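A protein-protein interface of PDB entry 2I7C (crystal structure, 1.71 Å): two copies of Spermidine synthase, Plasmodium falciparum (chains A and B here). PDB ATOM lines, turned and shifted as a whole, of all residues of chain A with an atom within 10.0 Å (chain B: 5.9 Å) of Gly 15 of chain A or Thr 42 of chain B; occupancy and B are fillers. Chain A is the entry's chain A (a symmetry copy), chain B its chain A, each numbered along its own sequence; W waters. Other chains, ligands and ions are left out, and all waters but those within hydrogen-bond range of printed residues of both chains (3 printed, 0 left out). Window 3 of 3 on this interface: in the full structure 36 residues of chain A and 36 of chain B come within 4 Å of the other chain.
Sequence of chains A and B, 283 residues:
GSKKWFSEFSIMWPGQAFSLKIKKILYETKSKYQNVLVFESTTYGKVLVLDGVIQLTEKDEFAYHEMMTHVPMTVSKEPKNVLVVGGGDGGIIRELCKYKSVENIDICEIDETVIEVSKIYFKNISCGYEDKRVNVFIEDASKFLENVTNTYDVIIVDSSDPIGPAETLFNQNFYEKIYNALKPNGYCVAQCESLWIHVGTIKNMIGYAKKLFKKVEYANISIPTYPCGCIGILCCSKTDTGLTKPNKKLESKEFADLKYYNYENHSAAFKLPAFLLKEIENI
Water W3 lies within hydrogen-bond range of the side-chain hydroxyl (OG) of Ser 19 of chain B and the backbone carbonyl oxygen (O) of Ala 17 of chain A.
Water W1 lies within hydrogen-bond range of the backbone carbonyl oxygen (O) of Gly 15 of chain A, the backbone NH (N) of Thr 43 of chain B, the side-chain hydroxyl (OG1) of Thr 42 of chain B and the backbone carbonyl oxygen (O) of Lys 21 of chain B.
Water W2 bridges OG1 of Thr 42 of chain B (2.9 Å) and N of Gly 15 of chain A (3.4 Å).
Phe 9 of chain A touches Trp 5 of chain B (CE1 to CH2, 3.7 Å).
Trp 5 of chain B touches Gly 15 of chain A.
Gly 15 of chain A touches Leu 20 of chain B.
Thr 42 of chain B touches Gly 15 of chain A.
Thr 43 of chain B touches Gly 15 of chain A (OG1 to CA, 3.8 Å).
C of Gln 16 of chain A touches CZ3 of Trp 5 of chain B, at 3.6 Å.
Gln 16 of chain A touches Ser 19 of chain B.
CZ3 of Trp 5 of chain B touches N of Ala 17 of chain A, at 3.8 Å.
Ile 197 of chain A touches Tyr 44 of chain B (CG2 to OH, 3.9 Å).
Hydrophobic or aromatic side chains of chain B that line the printed part of chain A: Trp 5, Leu 20 and Tyr 44.
Of the 13 printed residues of chain A, 7 touch a printed residue of chain B.
Printed residues of chain A that touch a printed residue of chain B: Phe 9, Pro 14, Gly 15, Gln 16, Ala 17, Ile 197 and Cys 228.
Hydrophobic or aromatic side chains of chain A that line the printed part of chain B: Phe 9 and Ile 197.
Among the printed residues, no Asp or Glu carboxylate lies within 4 Å of a Lys or Arg side-chain nitrogen of the other chain.
Printed residues of chain B within 4 Å of Gly 15 of chain A: Trp 5, Leu 20, Lys 21, Thr 42 and Thr 43.
Of chain A, only Gly 15 (3.5 Å) comes within 4 Å of Thr 42 of chain B.
No residue of chain A comes within 4 Å of Ser 41 of chain B.
Of the printed residues of chain B, Ile 197 of chain A touches Tyr 44.
Of the printed residues of chain A, Trp 5 of chain B touches Phe 9, Gly 15, Gln 16 and Ala 17.
The nearest residue of chain B that does not touch Gly 15 of chain A is Ser 19 of chain B (4.1 Å).
The nearest residue of chain A that does not touch Thr 42 of chain B is Pro 14 of chain A (5.1 Å).
The backbone NH (N) of Thr 42 of chain B sits at hydrogen-bond distance from the backbone carbonyl oxygen (O) of Lys 21 of chain B (2.9 Å).
The backbone NH (N) of Tyr 44 of chain B is in hydrogen-bond range of the side-chain hydroxyl (OG) of Ser 41 of chain B, 2.8 Å away.
NE2 of Gln 16 of chain A is in hydrogen-bond range of SG of Cys 228 of chain A, at 3.5 Å.
No position is printed for both chains.
The backbone carbonyl oxygen of Ala 17 of chain A sits at hydrogen-bond distance from the backbone NH of Ser 19 of chain B (2.7 Å).
The backbone carbonyl oxygen (O) of Gly 15 of chain A lies within hydrogen-bond range of the backbone NH (N) of Lys 21 of chain B, 2.9 Å away.
The backbone carbonyl oxygen of Pro 14 of chain A sits at hydrogen-bond distance from the side-chain hydroxyl of Thr 43 of chain B.
OE1 of Gln 16 of chain A lies within hydrogen-bond range of OH of Tyr 44 of chain B, 2.7 Å away.
OH of Tyr 44 of chain B lies within hydrogen-bond range of SG of Cys 228 of chain A (3.3 Å).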
ATOM      1  N   GLU A   8      28.651  27.476  15.874  1.00  0.00           N
ATOM      2  CA  GLU A   8      28.367  28.810  15.328  1.00  0.00           C
ATOM      3  C   GLU A   8      27.374  29.599  16.200  1.00  0.00           C
ATOM      4  O   GLU A   8      26.158  29.358  16.165  1.00  0.00           O
ATOM      5  CB  GLU A   8      27.836  28.692  13.894  1.00  0.00           C
ATOM      6  CG  GLU A   8      27.546  30.029  13.225  1.00  0.00           C
ATOM      7  CD  GLU A   8      26.749  29.885  11.945  1.00  0.00           C
ATOM      8  OE1 GLU A   8      25.680  29.226  11.986  1.00  0.00           O
ATOM      9  OE2 GLU A   8      27.175  30.450  10.907  1.00  0.00           O
ATOM     10  N   PHE A   9      27.908  30.543  16.971  1.00  0.00           N
ATOM     11  CA  PHE A   9      27.101  31.412  17.824  1.00  0.00           C
ATOM     12  C   PHE A   9      27.097  32.833  17.267  1.00  0.00           C
ATOM     13  O   PHE A   9      28.077  33.281  16.661  1.00  0.00           O
ATOM     14  CB  PHE A   9      27.661  31.442  19.255  1.00  0.00           C
ATOM     15  CG  PHE A   9      27.646  30.116  19.955  1.00  0.00           C
ATOM     16  CD1 PHE A   9      26.480  29.641  20.558  1.00  0.00           C
ATOM     17  CD2 PHE A   9      28.803  29.348  20.033  1.00  0.00           C
ATOM     18  CE1 PHE A   9      26.461  28.407  21.215  1.00  0.00           C
ATOM     19  CE2 PHE A   9      28.795  28.117  20.692  1.00  0.00           C
ATOM     20  CZ  PHE A   9      27.624  27.647  21.277  1.00  0.00           C
ATOM     21  N   SER A  10      25.982  33.535  17.462  1.00  0.00           N
ATOM     22  CA  SER A  10      25.883  34.953  17.119  1.00  0.00           C
ATOM     23  C   SER A  10      24.694  35.588  17.825  1.00  0.00           C
ATOM     24  O   SER A  10      23.675  34.928  18.087  1.00  0.00           O
ATOM     25  CB  SER A  10      25.767  35.152  15.604  1.00  0.00           C
ATOM     26  OG  SER A  10      25.655  36.517  15.239  1.00  0.00           O
ATOM     27  N   ILE A  11      24.836  36.870  18.142  1.00  0.00           N
ATOM     28  CA  ILE A  11      23.718  37.667  18.645  1.00  0.00           C
ATOM     29  C   ILE A  11      22.645  37.869  17.565  1.00  0.00           C
ATOM     30  O   ILE A  11      21.512  38.240  17.882  1.00  0.00           O
ATOM     31  CB  ILE A  11      24.173  39.033  19.238  1.00  0.00           C
ATOM     32  CG1 ILE A  11      24.887  39.876  18.181  1.00  0.00           C
ATOM     33  CG2 ILE A  11      25.043  38.806  20.479  1.00  0.00           C
ATOM     34  CD1 ILE A  11      24.795  41.376  18.428  1.00  0.00           C
ATOM     35  N   MET A  12      23.019  37.605  16.314  1.00  0.00           N
ATOM     36  CA  MET A  12      22.107  37.662  15.174  1.00  0.00           C
ATOM     37  C   MET A  12      21.154  36.452  15.133  1.00  0.00           C
ATOM     38  O   MET A  12      20.151  36.466  14.420  1.00  0.00           O
ATOM     39  CB  MET A  12      22.908  37.786  13.870  1.00  0.00           C
ATOM     40  CG  MET A  12      23.831  39.015  13.830  1.00  0.00           C
ATOM     41  SD  MET A  12      24.767  39.208  12.299  1.00  0.00           S
ATOM     42  CE  MET A  12      25.956  37.856  12.442  1.00  0.00           C
ATOM     43  N   TRP A  13      21.478  35.413  15.902  1.00  0.00           N
ATOM     44  CA  TRP A  13      20.583  34.259  16.108  1.00  0.00           C
ATOM     45  C   TRP A  13      20.684  33.749  17.552  1.00  0.00           C
ATOM     46  O   TRP A  13      21.250  32.688  17.812  1.00  0.00           O
ATOM     47  CB  TRP A  13      20.808  33.145  15.072  1.00  0.00           C
ATOM     48  CG  TRP A  13      22.241  32.852  14.682  1.00  0.00           C
ATOM     49  CD1 TRP A  13      23.075  31.946  15.254  1.00  0.00           C
ATOM     50  CD2 TRP A  13      22.977  33.451  13.602  1.00  0.00           C
ATOM     51  NE1 TRP A  13      24.289  31.938  14.607  1.00  0.00           N
ATOM     52  CE2 TRP A  13      24.258  32.855  13.589  1.00  0.00           C
ATOM     53  CE3 TRP A  13      22.677  34.439  12.654  1.00  0.00           C
ATOM     54  CZ2 TRP A  13      25.247  33.217  12.668  1.00  0.00           C
ATOM     55  CZ3 TRP A  13      23.658  34.798  11.720  1.00  0.00           C
ATOM     56  CH2 TRP A  13      24.929  34.192  11.741  1.00  0.00           C
ATOM     57  N   PRO A  14      20.128  34.521  18.501  1.00  0.00           N
ATOM     58  CA  PRO A  14      20.287  34.187  19.913  1.00  0.00           C
ATOM     59  C   PRO A  14      19.578  32.874  20.291  1.00  0.00           C
ATOM     60  O   PRO A  14      18.515  32.567  19.742  1.00  0.00           O
ATOM     61  CB  PRO A  14      19.638  35.380  20.629  1.00  0.00           C
ATOM     62  CG  PRO A  14      18.656  35.920  19.652  1.00  0.00           C
ATOM     63  CD  PRO A  14      19.308  35.736  18.307  1.00  0.00           C
ATOM     64  N   GLY A  15      20.170  32.103  21.200  1.00  0.00           N
ATOM     65  CA  GLY A  15      19.496  30.921  21.736  1.00  0.00           C
ATOM     66  C   GLY A  15      19.522  29.680  20.856  1.00  0.00           C
ATOM     67  O   GLY A  15      18.908  28.668  21.195  1.00  0.00           O
ATOM     68  N   GLN A  16      20.241  29.752  19.740  1.00  0.00           N
ATOM     69  CA  GLN A  16      20.421  28.609  18.844  1.00  0.00           C
ATOM     70  C   GLN A  16      21.860  28.524  18.364  1.00  0.00           C
ATOM     71  O   GLN A  16      22.570  29.541  18.298  1.00  0.00           O
ATOM     72  CB  GLN A  16      19.477  28.697  17.636  1.00  0.00           C
ATOM     73  CG  GLN A  16      19.799  29.847  16.654  1.00  0.00           C
ATOM     74  CD  GLN A  16      18.804  29.965  15.530  1.00  0.00           C
ATOM     75  OE1 GLN A  16      17.730  30.558  15.696  1.00  0.00           O
ATOM     76  NE2 GLN A  16      19.159  29.435  14.365  1.00  0.00           N
ATOM     77  N   ALA A  17      22.285  27.315  18.011  1.00  0.00           N
ATOM     78  CA  ALA A  17      23.611  27.108  17.406  1.00  0.00           C
ATOM     79  C   ALA A  17      23.653  25.858  16.541  1.00  0.00           C
ATOM     80  O   ALA A  17      23.022  24.846  16.852  1.00  0.00           O
ATOM     81  CB  ALA A  17      24.724  27.057  18.480  1.00  0.00           C
ATOM     82  N   PHE A  18      24.398  25.941  15.444  1.00  0.00           N
ATOM     83  CA  PHE A  18      24.654  24.795  14.578  1.00  0.00           C
ATOM     84  C   PHE A  18      26.125  24.412  14.760  1.00  0.00           C
ATOM     85  O   PHE A  18      26.989  25.294  14.868  1.00  0.00           O
ATOM     86  CB  PHE A  18      24.344  25.146  13.119  1.00  0.00           C
ATOM     87  CG  PHE A  18      24.641  24.042  12.150  1.00  0.00           C
ATOM     88  CD1 PHE A  18      23.873  22.883  12.144  1.00  0.00           C
ATOM     89  CD2 PHE A  18      25.690  24.153  11.242  1.00  0.00           C
ATOM     90  CE1 PHE A  18      24.147  21.852  11.245  1.00  0.00           C
ATOM     91  CE2 PHE A  18      25.968  23.131  10.335  1.00  0.00           C
ATOM     92  CZ  PHE A  18      25.191  21.978  10.340  1.00  0.00           C
ATOM     93  N   ILE A 197      14.074  33.993  11.425  1.00  0.00           N
ATOM     94  CA  ILE A 197      14.574  34.770  12.559  1.00  0.00           C
ATOM     95  C   ILE A 197      14.856  36.249  12.270  1.00  0.00           C
ATOM     96  O   ILE A 197      15.033  37.029  13.206  1.00  0.00           O
ATOM     97  CB  ILE A 197      15.836  34.120  13.196  1.00  0.00           C
ATOM     98  CG1 ILE A 197      16.859  33.760  12.104  1.00  0.00           C
ATOM     99  CG2 ILE A 197      15.447  32.914  14.077  1.00  0.00           C
ATOM    100  CD1 ILE A 197      18.212  33.300  12.623  1.00  0.00           C
ATOM    101  N   CYS A 228      19.100  28.494  10.613  1.00  0.00           N
ATOM    102  CA  CYS A 228      17.720  28.112  10.310  1.00  0.00           C
ATOM    103  C   CYS A 228      17.563  27.290   9.011  1.00  0.00           C
ATOM    104  O   CYS A 228      16.445  26.945   8.634  1.00  0.00           O
ATOM    105  CB  CYS A 228      16.776  29.326  10.352  1.00  0.00           C
ATOM    106  SG  CYS A 228      16.632  30.034  12.011  1.00  0.00           S
ATOM    107  N   LYS B   3      22.821  29.539  31.876  1.00  0.00           N
ATOM    108  CA  LYS B   3      21.847  28.640  31.180  1.00  0.00           C
ATOM    109  C   LYS B   3      22.569  27.558  30.373  1.00  0.00           C
ATOM    110  O   LYS B   3      23.552  27.840  29.685  1.00  0.00           O
ATOM    111  CB  LYS B   3      20.904  29.457  30.279  1.00  0.00           C
ATOM    112  CG  LYS B   3      19.781  30.171  31.042  1.00  0.00           C
ATOM    113  CD  LYS B   3      18.876  30.970  30.104  1.00  0.00           C
ATOM    114  CE  LYS B   3      17.787  31.719  30.873  1.00  0.00           C
ATOM    115  NZ  LYS B   3      18.333  32.833  31.705  1.00  0.00           N
ATOM    116  N   TRP B   5      22.568  24.304  27.459  1.00  0.00           N
ATOM    117  CA  TRP B   5      22.076  24.116  26.099  1.00  0.00           C
ATOM    118  C   TRP B   5      21.659  22.665  25.874  1.00  0.00           C
ATOM    119  O   TRP B   5      22.304  21.744  26.387  1.00  0.00           O
ATOM    120  CB  TRP B   5      23.182  24.470  25.101  1.00  0.00           C
ATOM    121  CG  TRP B   5      23.497  25.942  25.003  1.00  0.00           C
ATOM    122  CD1 TRP B   5      24.147  26.721  25.931  1.00  0.00           C
ATOM    123  CD2 TRP B   5      23.203  26.803  23.898  1.00  0.00           C
ATOM    124  NE1 TRP B   5      24.253  28.018  25.475  1.00  0.00           N
ATOM    125  CE2 TRP B   5      23.681  28.097  24.232  1.00  0.00           C
ATOM    126  CE3 TRP B   5      22.565  26.616  22.665  1.00  0.00           C
ATOM    127  CZ2 TRP B   5      23.548  29.194  23.363  1.00  0.00           C
ATOM    128  CZ3 TRP B   5      22.443  27.709  21.799  1.00  0.00           C
ATOM    129  CH2 TRP B   5      22.929  28.977  22.156  1.00  0.00           C
ATOM    130  N   SER B  19      21.620  23.045  18.320  1.00  0.00           N
ATOM    131  CA  SER B  19      21.446  23.275  19.748  1.00  0.00           C
ATOM    132  C   SER B  19      20.460  24.397  20.065  1.00  0.00           C
ATOM    133  O   SER B  19      20.379  25.370  19.333  1.00  0.00           O
ATOM    134  CB  SER B  19      22.789  23.597  20.404  1.00  0.00           C
ATOM    135  OG  SER B  19      23.690  22.511  20.302  1.00  0.00           O
ATOM    136  N   LEU B  20      19.733  24.252  21.178  1.00  0.00           N
ATOM    137  CA  LEU B  20      18.844  25.302  21.676  1.00  0.00           C
ATOM    138  C   LEU B  20      19.182  25.634  23.129  1.00  0.00           C
ATOM    139  O   LEU B  20      19.373  24.731  23.943  1.00  0.00           O
ATOM    140  CB  LEU B  20      17.383  24.858  21.588  1.00  0.00           C
ATOM    141  CG  LEU B  20      16.771  24.808  20.185  1.00  0.00           C
ATOM    142  CD1 LEU B  20      15.400  24.198  20.290  1.00  0.00           C
ATOM    143  CD2 LEU B  20      16.709  26.195  19.547  1.00  0.00           C
ATOM    144  N   LYS B  21      19.242  26.921  23.457  1.00  0.00           N
ATOM    145  CA  LYS B  21      19.495  27.328  24.840  1.00  0.00           C
ATOM    146  C   LYS B  21      18.246  27.052  25.679  1.00  0.00           C
ATOM    147  O   LYS B  21      17.121  27.348  25.254  1.00  0.00           O
ATOM    148  CB  LYS B  21      19.908  28.798  24.912  1.00  0.00           C
ATOM    149  CG  LYS B  21      20.377  29.236  26.295  1.00  0.00           C
ATOM    150  CD  LYS B  21      20.680  30.726  26.307  1.00  0.00           C
ATOM    151  CE  LYS B  21      22.155  31.012  26.276  1.00  0.00           C
ATOM    152  NZ  LYS B  21      22.406  32.450  26.621  1.00  0.00           N
ATOM    153  N   ILE B  22      18.468  26.482  26.865  1.00  0.00           N
ATOM    154  CA  ILE B  22      17.397  26.054  27.781  1.00  0.00           C
ATOM    155  C   ILE B  22      17.096  27.154  28.786  1.00  0.00           C
ATOM    156  O   ILE B  22      17.979  27.553  29.558  1.00  0.00           O
ATOM    157  CB  ILE B  22      17.798  24.753  28.540  1.00  0.00           C
ATOM    158  CG1 ILE B  22      18.094  23.618  27.558  1.00  0.00           C
ATOM    159  CG2 ILE B  22      16.715  24.327  29.559  1.00  0.00           C
ATOM    160  CD1 ILE B  22      18.905  22.459  28.154  1.00  0.00           C
ATOM    161  N   LYS B  23      15.864  27.654  28.767  1.00  0.00           N
ATOM    162  CA  LYS B  23      15.397  28.565  29.810  1.00  0.00           C
ATOM    163  C   LYS B  23      15.121  27.746  31.074  1.00  0.00           C
ATOM    164  O   LYS B  23      15.589  28.096  32.166  1.00  0.00           O
ATOM    165  CB  LYS B  23      14.157  29.336  29.362  1.00  0.00           C
ATOM    166  CG  LYS B  23      13.733  30.448  30.317  1.00  0.00           C
ATOM    167  CD  LYS B  23      12.493  31.177  29.815  1.00  0.00           C
ATOM    168  CE  LYS B  23      12.261  32.477  30.595  1.00  0.00           C
ATOM    169  NZ  LYS B  23      10.796  32.799  30.687  1.00  0.00           N
ATOM    170  N   GLU B  40      11.454  24.493  28.188  1.00  0.00           N
ATOM    171  CA  GLU B  40      11.249  25.811  27.610  1.00  0.00           C
ATOM    172  C   GLU B  40      12.597  26.319  27.114  1.00  0.00           C
ATOM    173  O   GLU B  40      13.555  26.470  27.893  1.00  0.00           O
ATOM    174  CB  GLU B  40      10.616  26.801  28.600  1.00  0.00           C
ATOM    175  CG  GLU B  40      10.340  28.181  27.956  1.00  0.00           C
ATOM    176  CD  GLU B  40       9.751  29.224  28.906  1.00  0.00           C
ATOM    177  OE1 GLU B  40       9.754  29.014  30.141  1.00  0.00           O
ATOM    178  OE2 GLU B  40       9.290  30.275  28.404  1.00  0.00           O
ATOM    179  N   SER B  41      12.678  26.551  25.809  1.00  0.00           N
ATOM    180  CA  SER B  41      13.877  27.119  25.214  1.00  0.00           C
ATOM    181  C   SER B  41      13.830  28.639  25.415  1.00  0.00           C
ATOM    182  O   SER B  41      12.784  29.198  25.773  1.00  0.00           O
ATOM    183  CB  SER B  41      13.959  26.769  23.715  1.00  0.00           C
ATOM    184  OG  SER B  41      12.967  27.470  22.967  1.00  0.00           O
ATOM    185  N   THR B  42      14.949  29.315  25.177  1.00  0.00           N
ATOM    186  CA  THR B  42      14.983  30.767  25.333  1.00  0.00           C
ATOM    187  C   THR B  42      14.296  31.481  24.156  1.00  0.00           C
ATOM    188  O   THR B  42      13.702  32.551  24.334  1.00  0.00           O
ATOM    189  CB  THR B  42      16.441  31.298  25.516  1.00  0.00           C
ATOM    190  OG1 THR B  42      17.243  30.886  24.409  1.00  0.00           O
ATOM    191  CG2 THR B  42      17.067  30.755  26.789  1.00  0.00           C
ATOM    192  N   THR B  43      14.381  30.913  22.955  1.00  0.00           N
ATOM    193  CA  THR B  43      13.901  31.649  21.783  1.00  0.00           C
ATOM    194  C   THR B  43      12.924  30.898  20.874  1.00  0.00           C
ATOM    195  O   THR B  43      12.330  31.511  19.985  1.00  0.00           O
ATOM    196  CB  THR B  43      15.068  32.275  20.964  1.00  0.00           C
ATOM    197  OG1 THR B  43      15.924  31.238  20.471  1.00  0.00           O
ATOM    198  CG2 THR B  43      15.887  33.241  21.828  1.00  0.00           C
ATOM    199  N   TYR B  44      12.729  29.600  21.123  1.00  0.00           N
ATOM    200  CA  TYR B  44      11.847  28.764  20.293  1.00  0.00           C
ATOM    201  C   TYR B  44      10.605  28.256  21.041  1.00  0.00           C
ATOM    202  O   TYR B  44       9.850  27.407  20.527  1.00  0.00           O
ATOM    203  CB  TYR B  44      12.630  27.598  19.648  1.00  0.00           C
ATOM    204  CG  TYR B  44      13.410  27.997  18.395  1.00  0.00           C
ATOM    205  CD1 TYR B  44      14.565  28.778  18.488  1.00  0.00           C
ATOM    206  CD2 TYR B  44      12.975  27.618  17.123  1.00  0.00           C
ATOM    207  CE1 TYR B  44      15.285  29.155  17.343  1.00  0.00           C
ATOM    208  CE2 TYR B  44      13.689  28.001  15.965  1.00  0.00           C
ATOM    209  CZ  TYR B  44      14.836  28.775  16.090  1.00  0.00           C
ATOM    210  OH  TYR B  44      15.549  29.161  14.966  1.00  0.00           O
ATOM    211  N   GLY B  45      10.375  28.800  22.235  1.00  0.00           N
ATOM    212  CA  GLY B  45       9.244  28.367  23.052  1.00  0.00           C
ATOM    213  C   GLY B  45       9.478  26.974  23.612  1.00  0.00           C
ATOM    214  O   GLY B  45      10.627  26.549  23.761  1.00  0.00           O
HETATM  215  O   HOH W   1      16.265  28.709  22.289  1.00  0.00           O
HETATM  216  O   HOH W   2      18.788  33.282  24.061  1.00  0.00           O
HETATM  217  O   HOH W   3      25.030  22.853  17.955  1.00  0.00           O
